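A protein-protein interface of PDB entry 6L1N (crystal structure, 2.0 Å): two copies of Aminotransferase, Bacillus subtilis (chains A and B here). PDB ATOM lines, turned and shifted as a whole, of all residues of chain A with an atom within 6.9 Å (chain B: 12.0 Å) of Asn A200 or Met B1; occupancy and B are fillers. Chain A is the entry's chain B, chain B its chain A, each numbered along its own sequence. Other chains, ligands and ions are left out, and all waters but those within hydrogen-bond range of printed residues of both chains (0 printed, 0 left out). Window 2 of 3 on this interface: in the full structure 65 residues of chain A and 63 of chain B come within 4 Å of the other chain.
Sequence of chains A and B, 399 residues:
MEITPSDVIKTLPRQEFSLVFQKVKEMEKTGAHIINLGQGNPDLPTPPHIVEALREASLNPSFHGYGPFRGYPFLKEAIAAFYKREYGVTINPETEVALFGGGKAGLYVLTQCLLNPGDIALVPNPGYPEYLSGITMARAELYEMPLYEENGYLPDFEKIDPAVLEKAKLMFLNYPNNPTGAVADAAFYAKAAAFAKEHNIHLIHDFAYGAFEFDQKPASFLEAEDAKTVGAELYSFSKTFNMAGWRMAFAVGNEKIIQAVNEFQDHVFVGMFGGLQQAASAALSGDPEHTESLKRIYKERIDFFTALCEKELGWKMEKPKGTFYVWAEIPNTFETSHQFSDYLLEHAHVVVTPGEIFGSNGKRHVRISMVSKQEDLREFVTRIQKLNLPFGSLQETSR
A ring nitrogen (NE2) of His A202 sits at hydrogen-bond distance from the backbone NH of Ile B3 (3.1 Å).
The backbone NH (N) of His A202 is in hydrogen-bond range of the backbone carbonyl oxygen (O) of Lys A169 (2.9 Å).
Asn A200 touches Met B1 (OD1 to N, 3.7 Å).
CA of Glu B2 touches NE2 of His A202, at 3.7 Å.
CD of Glu B2 touches O of Thr A229, 3.3 Å away.
O of Val A230 touches OE1 of Glu B2, 3.6 Å away.
Asn A200 touches just one residue of chain B: Met B1.
Met B1 touches just one residue of chain A: Asn A200.
Ala A168 touches none of the printed residues of chain B.
Ala A196 touches none of the printed residues of chain B.
No residue of chain B comes within 4 Å of Lys A197.
No residue of chain B comes within 4 Å of Glu A198.
His A199 touches none of the printed residues of chain B.
No residue of chain B comes within 4 Å of Ile A201.
Printed residues of chain B within 4 Å of Val A230: Glu B2.
Of the printed residues of chain A, Glu B2 touches His A202 (3.7 Å), Thr A229 (3.3 Å) and Val A230 (3.6 Å).
Of the printed residues of chain B, Thr A229 touches Glu B2.
Of the printed residues of chain A, Ile B3 touches His A202.
Phe A195 touches none of the printed residues of chain B.
Leu A170 touches none of the printed residues of chain B.
The nearest residue of chain A that does not touch Met B1 is His A202 (4.4 Å).
The nearest printed residue of chain B that does not touch Thr A229 is Met B1 (6.1 Å).
Hydrophobic or aromatic side chains of chain A that line the printed part of chain B: His A202.
Of the 7 printed residues of chain B, 3 touch a printed residue of chain A.
Along chain B the printed residues that touch a printed residue of chain A span positions 1 to 3.
Among the printed residues, no Asp or Glu carboxylate lies within 4 Å of a Lys or Arg side-chain nitrogen of the other chain.
No position is printed for both chains.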
ATOM      1  N   LEU A 165     -23.087   4.246  18.476  1.00  0.00           N
ATOM      2  CA  LEU A 165     -22.629   3.238  17.529  1.00  0.00           C
ATOM      3  C   LEU A 165     -22.008   2.013  18.148  1.00  0.00           C
ATOM      4  O   LEU A 165     -21.985   0.968  17.516  1.00  0.00           O
ATOM      5  CB  LEU A 165     -21.695   3.854  16.561  1.00  0.00           C
ATOM      6  CG  LEU A 165     -22.358   5.018  15.788  1.00  0.00           C
ATOM      7  CD1 LEU A 165     -21.394   5.998  15.129  1.00  0.00           C
ATOM      8  CD2 LEU A 165     -23.339   4.552  14.763  1.00  0.00           C
ATOM      9  N   GLU A 166     -21.517   2.132  19.378  1.00  0.00           N
ATOM     10  CA  GLU A 166     -21.021   1.002  20.147  1.00  0.00           C
ATOM     11  C   GLU A 166     -22.174   0.054  20.507  1.00  0.00           C
ATOM     12  O   GLU A 166     -21.999  -1.164  20.591  1.00  0.00           O
ATOM     13  CB  GLU A 166     -20.277   1.474  21.424  1.00  0.00           C
ATOM     14  N   LYS A 167     -23.347   0.631  20.745  1.00  0.00           N
ATOM     15  CA  LYS A 167     -24.507  -0.136  21.082  1.00  0.00           C
ATOM     16  C   LYS A 167     -25.408  -0.386  19.892  1.00  0.00           C
ATOM     17  O   LYS A 167     -26.303  -1.223  19.978  1.00  0.00           O
ATOM     18  CB  LYS A 167     -25.277   0.630  22.171  1.00  0.00           C
ATOM     19  N   ALA A 168     -25.293   0.398  18.824  1.00  0.00           N
ATOM     20  CA  ALA A 168     -26.229   0.212  17.686  1.00  0.00           C
ATOM     21  C   ALA A 168     -26.039  -1.151  17.048  1.00  0.00           C
ATOM     22  O   ALA A 168     -24.920  -1.517  16.701  1.00  0.00           O
ATOM     23  CB  ALA A 168     -26.067   1.281  16.637  1.00  0.00           C
ATOM     24  N   LYS A 169     -27.130  -1.900  16.906  1.00  0.00           N
ATOM     25  CA  LYS A 169     -27.085  -3.229  16.324  1.00  0.00           C
ATOM     26  C   LYS A 169     -27.686  -3.279  14.928  1.00  0.00           C
ATOM     27  O   LYS A 169     -27.404  -4.197  14.138  1.00  0.00           O
ATOM     28  CB  LYS A 169     -27.826  -4.211  17.243  1.00  0.00           C
ATOM     29  N   LEU A 170     -28.601  -2.352  14.650  1.00  0.00           N
ATOM     30  CA  LEU A 170     -29.332  -2.332  13.400  1.00  0.00           C
ATOM     31  C   LEU A 170     -29.538  -0.914  12.886  1.00  0.00           C
ATOM     32  O   LEU A 170     -29.762   0.005  13.655  1.00  0.00           O
ATOM     33  CB  LEU A 170     -30.719  -2.992  13.625  1.00  0.00           C
ATOM     34  CG  LEU A 170     -31.692  -3.162  12.448  1.00  0.00           C
ATOM     35  CD1 LEU A 170     -31.083  -4.156  11.482  1.00  0.00           C
ATOM     36  CD2 LEU A 170     -33.056  -3.677  12.934  1.00  0.00           C
ATOM     37  N   PHE A 195     -19.505   2.101   6.870  1.00  0.00           N
ATOM     38  CA  PHE A 195     -19.880   2.562   8.169  1.00  0.00           C
ATOM     39  C   PHE A 195     -20.424   1.452   9.086  1.00  0.00           C
ATOM     40  O   PHE A 195     -20.058   1.341  10.279  1.00  0.00           O
ATOM     41  CB  PHE A 195     -20.945   3.628   7.994  1.00  0.00           C
ATOM     42  CG  PHE A 195     -21.282   4.324   9.231  1.00  0.00           C
ATOM     43  CD1 PHE A 195     -20.472   5.368   9.679  1.00  0.00           C
ATOM     44  CD2 PHE A 195     -22.411   3.945   9.974  1.00  0.00           C
ATOM     45  CE1 PHE A 195     -20.780   6.028  10.851  1.00  0.00           C
ATOM     46  CE2 PHE A 195     -22.719   4.620  11.150  1.00  0.00           C
ATOM     47  CZ  PHE A 195     -21.922   5.650  11.578  1.00  0.00           C
ATOM     48  N   ALA A 196     -21.302   0.642   8.526  1.00  0.00           N
ATOM     49  CA  ALA A 196     -21.888  -0.495   9.245  1.00  0.00           C
ATOM     50  C   ALA A 196     -20.824  -1.529   9.637  1.00  0.00           C
ATOM     51  O   ALA A 196     -20.840  -2.041  10.724  1.00  0.00           O
ATOM     52  CB  ALA A 196     -22.941  -1.133   8.385  1.00  0.00           C
ATOM     53  N   LYS A 197     -19.879  -1.779   8.741  1.00  0.00           N
ATOM     54  CA  LYS A 197     -18.815  -2.749   8.991  1.00  0.00           C
ATOM     55  C   LYS A 197     -17.908  -2.269  10.126  1.00  0.00           C
ATOM     56  O   LYS A 197     -17.573  -3.039  11.002  1.00  0.00           O
ATOM     57  CB  LYS A 197     -17.984  -2.932   7.731  1.00  0.00           C
ATOM     58  CG  LYS A 197     -16.996  -4.076   7.823  1.00  0.00           C
ATOM     59  CD  LYS A 197     -16.229  -4.286   6.539  1.00  0.00           C
ATOM     60  CE  LYS A 197     -15.660  -5.697   6.446  1.00  0.00           C
ATOM     61  NZ  LYS A 197     -14.375  -5.872   7.180  1.00  0.00           N
ATOM     62  N   GLU A 198     -17.548  -0.981  10.120  1.00  0.00           N
ATOM     63  CA  GLU A 198     -16.709  -0.439  11.158  1.00  0.00           C
ATOM     64  C   GLU A 198     -17.296  -0.560  12.576  1.00  0.00           C
ATOM     65  O   GLU A 198     -16.567  -0.779  13.541  1.00  0.00           O
ATOM     66  CB  GLU A 198     -16.347   1.014  10.872  1.00  0.00           C
ATOM     67  N   HIS A 199     -18.615  -0.396  12.649  1.00  0.00           N
ATOM     68  CA  HIS A 199     -19.357  -0.222  13.873  1.00  0.00           C
ATOM     69  C   HIS A 199     -20.152  -1.492  14.221  1.00  0.00           C
ATOM     70  O   HIS A 199     -20.843  -1.516  15.184  1.00  0.00           O
ATOM     71  CB  HIS A 199     -20.250   0.997  13.650  1.00  0.00           C
ATOM     72  CG  HIS A 199     -19.486   2.283  13.530  1.00  0.00           C
ATOM     73  ND1 HIS A 199     -18.292   2.426  12.862  1.00  0.00           N
ATOM     74  CD2 HIS A 199     -19.780   3.509  13.990  1.00  0.00           C
ATOM     75  CE1 HIS A 199     -17.873   3.678  12.942  1.00  0.00           C
ATOM     76  NE2 HIS A 199     -18.764   4.360  13.617  1.00  0.00           N
ATOM     77  N   ASN A 200     -19.960  -2.555  13.429  1.00  0.00           N
ATOM     78  CA  ASN A 200     -20.711  -3.813  13.499  1.00  0.00           C
ATOM     79  C   ASN A 200     -22.207  -3.559  13.643  1.00  0.00           C
ATOM     80  O   ASN A 200     -22.798  -3.934  14.650  1.00  0.00           O
ATOM     81  CB  ASN A 200     -20.184  -4.694  14.632  1.00  0.00           C
ATOM     82  CG  ASN A 200     -18.739  -5.110  14.392  1.00  0.00           C
ATOM     83  OD1 ASN A 200     -18.416  -5.676  13.351  1.00  0.00           O
ATOM     84  ND2 ASN A 200     -17.872  -4.791  15.314  1.00  0.00           N
ATOM     85  N   ILE A 201     -22.777  -2.846  12.654  1.00  0.00           N
ATOM     86  CA  ILE A 201     -24.198  -2.582  12.601  1.00  0.00           C
ATOM     87  C   ILE A 201     -24.748  -3.419  11.431  1.00  0.00           C
ATOM     88  O   ILE A 201     -24.120  -3.493  10.403  1.00  0.00           O
ATOM     89  CB  ILE A 201     -24.473  -1.078  12.401  1.00  0.00           C
ATOM     90  CG1 ILE A 201     -23.855  -0.253  13.560  1.00  0.00           C
ATOM     91  CG2 ILE A 201     -25.960  -0.826  12.387  1.00  0.00           C
ATOM     92  CD1 ILE A 201     -23.915   1.251  13.360  1.00  0.00           C
ATOM     93  N   HIS A 202     -25.866  -4.110  11.655  1.00  0.00           N
ATOM     94  CA  HIS A 202     -26.592  -4.850  10.624  1.00  0.00           C
ATOM     95  C   HIS A 202     -27.352  -3.812   9.801  1.00  0.00           C
ATOM     96  O   HIS A 202     -28.032  -2.933  10.366  1.00  0.00           O
ATOM     97  CB  HIS A 202     -27.615  -5.795  11.247  1.00  0.00           C
ATOM     98  CG  HIS A 202     -27.005  -6.918  12.009  1.00  0.00           C
ATOM     99  ND1 HIS A 202     -27.747  -7.894  12.619  1.00  0.00           N
ATOM    100  CD2 HIS A 202     -25.718  -7.230  12.239  1.00  0.00           C
ATOM    101  CE1 HIS A 202     -26.946  -8.776  13.185  1.00  0.00           C
ATOM    102  NE2 HIS A 202     -25.711  -8.381  12.986  1.00  0.00           N
ATOM    103  N   THR A 229     -21.689  -8.271   3.212  1.00  0.00           N
ATOM    104  CA  THR A 229     -21.004  -8.567   4.422  1.00  0.00           C
ATOM    105  C   THR A 229     -21.756  -8.072   5.681  1.00  0.00           C
ATOM    106  O   THR A 229     -21.562  -8.601   6.786  1.00  0.00           O
ATOM    107  CB  THR A 229     -19.581  -7.918   4.354  1.00  0.00           C
ATOM    108  OG1 THR A 229     -18.805  -8.559   3.340  1.00  0.00           O
ATOM    109  CG2 THR A 229     -18.808  -8.084   5.645  1.00  0.00           C
ATOM    110  N   VAL A 230     -22.553  -7.003   5.543  1.00  0.00           N
ATOM    111  CA  VAL A 230     -23.137  -6.325   6.719  1.00  0.00           C
ATOM    112  C   VAL A 230     -24.662  -6.327   6.770  1.00  0.00           C
ATOM    113  O   VAL A 230     -25.194  -5.930   7.767  1.00  0.00           O
ATOM    114  CB  VAL A 230     -22.668  -4.853   6.784  1.00  0.00           C
ATOM    115  CG1 VAL A 230     -21.176  -4.772   6.912  1.00  0.00           C
ATOM    116  CG2 VAL A 230     -23.115  -4.030   5.564  1.00  0.00           C
ATOM    117  N   MET B   1     -18.789  -9.338  13.086  1.00  0.00           N
ATOM    118  CA  MET B   1     -19.552 -10.471  12.478  1.00  0.00           C
ATOM    119  C   MET B   1     -21.066 -10.265  12.628  1.00  0.00           C
ATOM    120  O   MET B   1     -21.550  -9.630  13.593  1.00  0.00           O
ATOM    121  CB  MET B   1     -19.150 -11.802  13.124  1.00  0.00           C
ATOM    122  N   GLU B   2     -21.816 -10.814  11.671  1.00  0.00           N
ATOM    123  CA  GLU B   2     -23.290 -10.874  11.789  1.00  0.00           C
ATOM    124  C   GLU B   2     -23.610 -11.601  13.087  1.00  0.00           C
ATOM    125  O   GLU B   2     -23.130 -12.693  13.293  1.00  0.00           O
ATOM    126  CB  GLU B   2     -23.919 -11.616  10.604  1.00  0.00           C
ATOM    127  CG  GLU B   2     -23.438 -11.126   9.254  1.00  0.00           C
ATOM    128  CD  GLU B   2     -23.659  -9.649   9.045  1.00  0.00           C
ATOM    129  OE1 GLU B   2     -24.821  -9.215   9.171  1.00  0.00           O
ATOM    130  N   ILE B   3     -24.337 -10.950  13.991  1.00  0.00           N
ATOM    131  CA  ILE B   3     -24.765 -11.536  15.264  1.00  0.00           C
ATOM    132  C   ILE B   3     -26.249 -11.341  15.476  1.00  0.00           C
ATOM    133  O   ILE B   3     -26.691 -10.315  15.959  1.00  0.00           O
ATOM    134  CB  ILE B   3     -23.941 -10.986  16.448  1.00  0.00           C
ATOM    135  CG1 ILE B   3     -22.470 -11.391  16.313  1.00  0.00           C
ATOM    136  CG2 ILE B   3     -24.492 -11.480  17.792  1.00  0.00           C
ATOM    137  CD1 ILE B   3     -22.161 -12.885  16.298  1.00  0.00           C
ATOM    138  N   THR B   4     -26.993 -12.348  15.063  1.00  0.00           N
ATOM    139  CA  THR B   4     -28.422 -12.554  15.338  1.00  0.00           C
ATOM    140  C   THR B   4     -28.791 -12.466  16.836  1.00  0.00           C
ATOM    141  O   THR B   4     -27.919 -12.708  17.653  1.00  0.00           O
ATOM    142  CB  THR B   4     -28.642 -13.971  14.844  1.00  0.00           C
ATOM    143  OG1 THR B   4     -27.942 -14.121  13.576  1.00  0.00           O
ATOM    144  CG2 THR B   4     -30.098 -14.300  14.715  1.00  0.00           C
ATOM    145  N   PRO B   5     -30.055 -12.128  17.229  1.00  0.00           N
ATOM    146  CA  PRO B   5     -30.304 -12.143  18.642  1.00  0.00           C
ATOM    147  C   PRO B   5     -30.324 -13.560  19.119  1.00  0.00           C
ATOM    148  O   PRO B   5     -30.611 -14.463  18.329  1.00  0.00           O
ATOM    149  CB  PRO B   5     -31.695 -11.523  18.778  1.00  0.00           C
ATOM    150  CG  PRO B   5     -32.392 -11.995  17.636  1.00  0.00           C
ATOM    151  CD  PRO B   5     -31.310 -11.792  16.569  1.00  0.00           C
ATOM    152  N   SER B   6     -30.000 -13.721  20.392  1.00  0.00           N
ATOM    153  CA  SER B   6     -29.718 -15.029  20.984  1.00  0.00           C
ATOM    154  C   SER B   6     -30.941 -15.948  20.949  1.00  0.00           C
ATOM    155  O   SER B   6     -30.818 -17.137  20.662  1.00  0.00           O
ATOM    156  CB  SER B   6     -29.187 -14.828  22.406  1.00  0.00           C
ATOM    157  OG  SER B   6     -29.613 -13.567  22.903  1.00  0.00           O
ATOM    158  N   ILE B   9     -31.929 -18.976  18.088  1.00  0.00           N
ATOM    159  CA  ILE B   9     -31.332 -20.343  18.093  1.00  0.00           C
ATOM    160  C   ILE B   9     -31.629 -21.023  19.474  1.00  0.00           C
ATOM    161  O   ILE B   9     -31.401 -22.235  19.693  1.00  0.00           O
ATOM    162  CB  ILE B   9     -29.833 -20.349  17.630  1.00  0.00           C
ATOM    163  CG1 ILE B   9     -29.608 -19.434  16.389  1.00  0.00           C
ATOM    164  CG2 ILE B   9     -29.366 -21.755  17.232  1.00  0.00           C
ATOM    165  CD1 ILE B   9     -29.257 -17.964  16.666  1.00  0.00           C
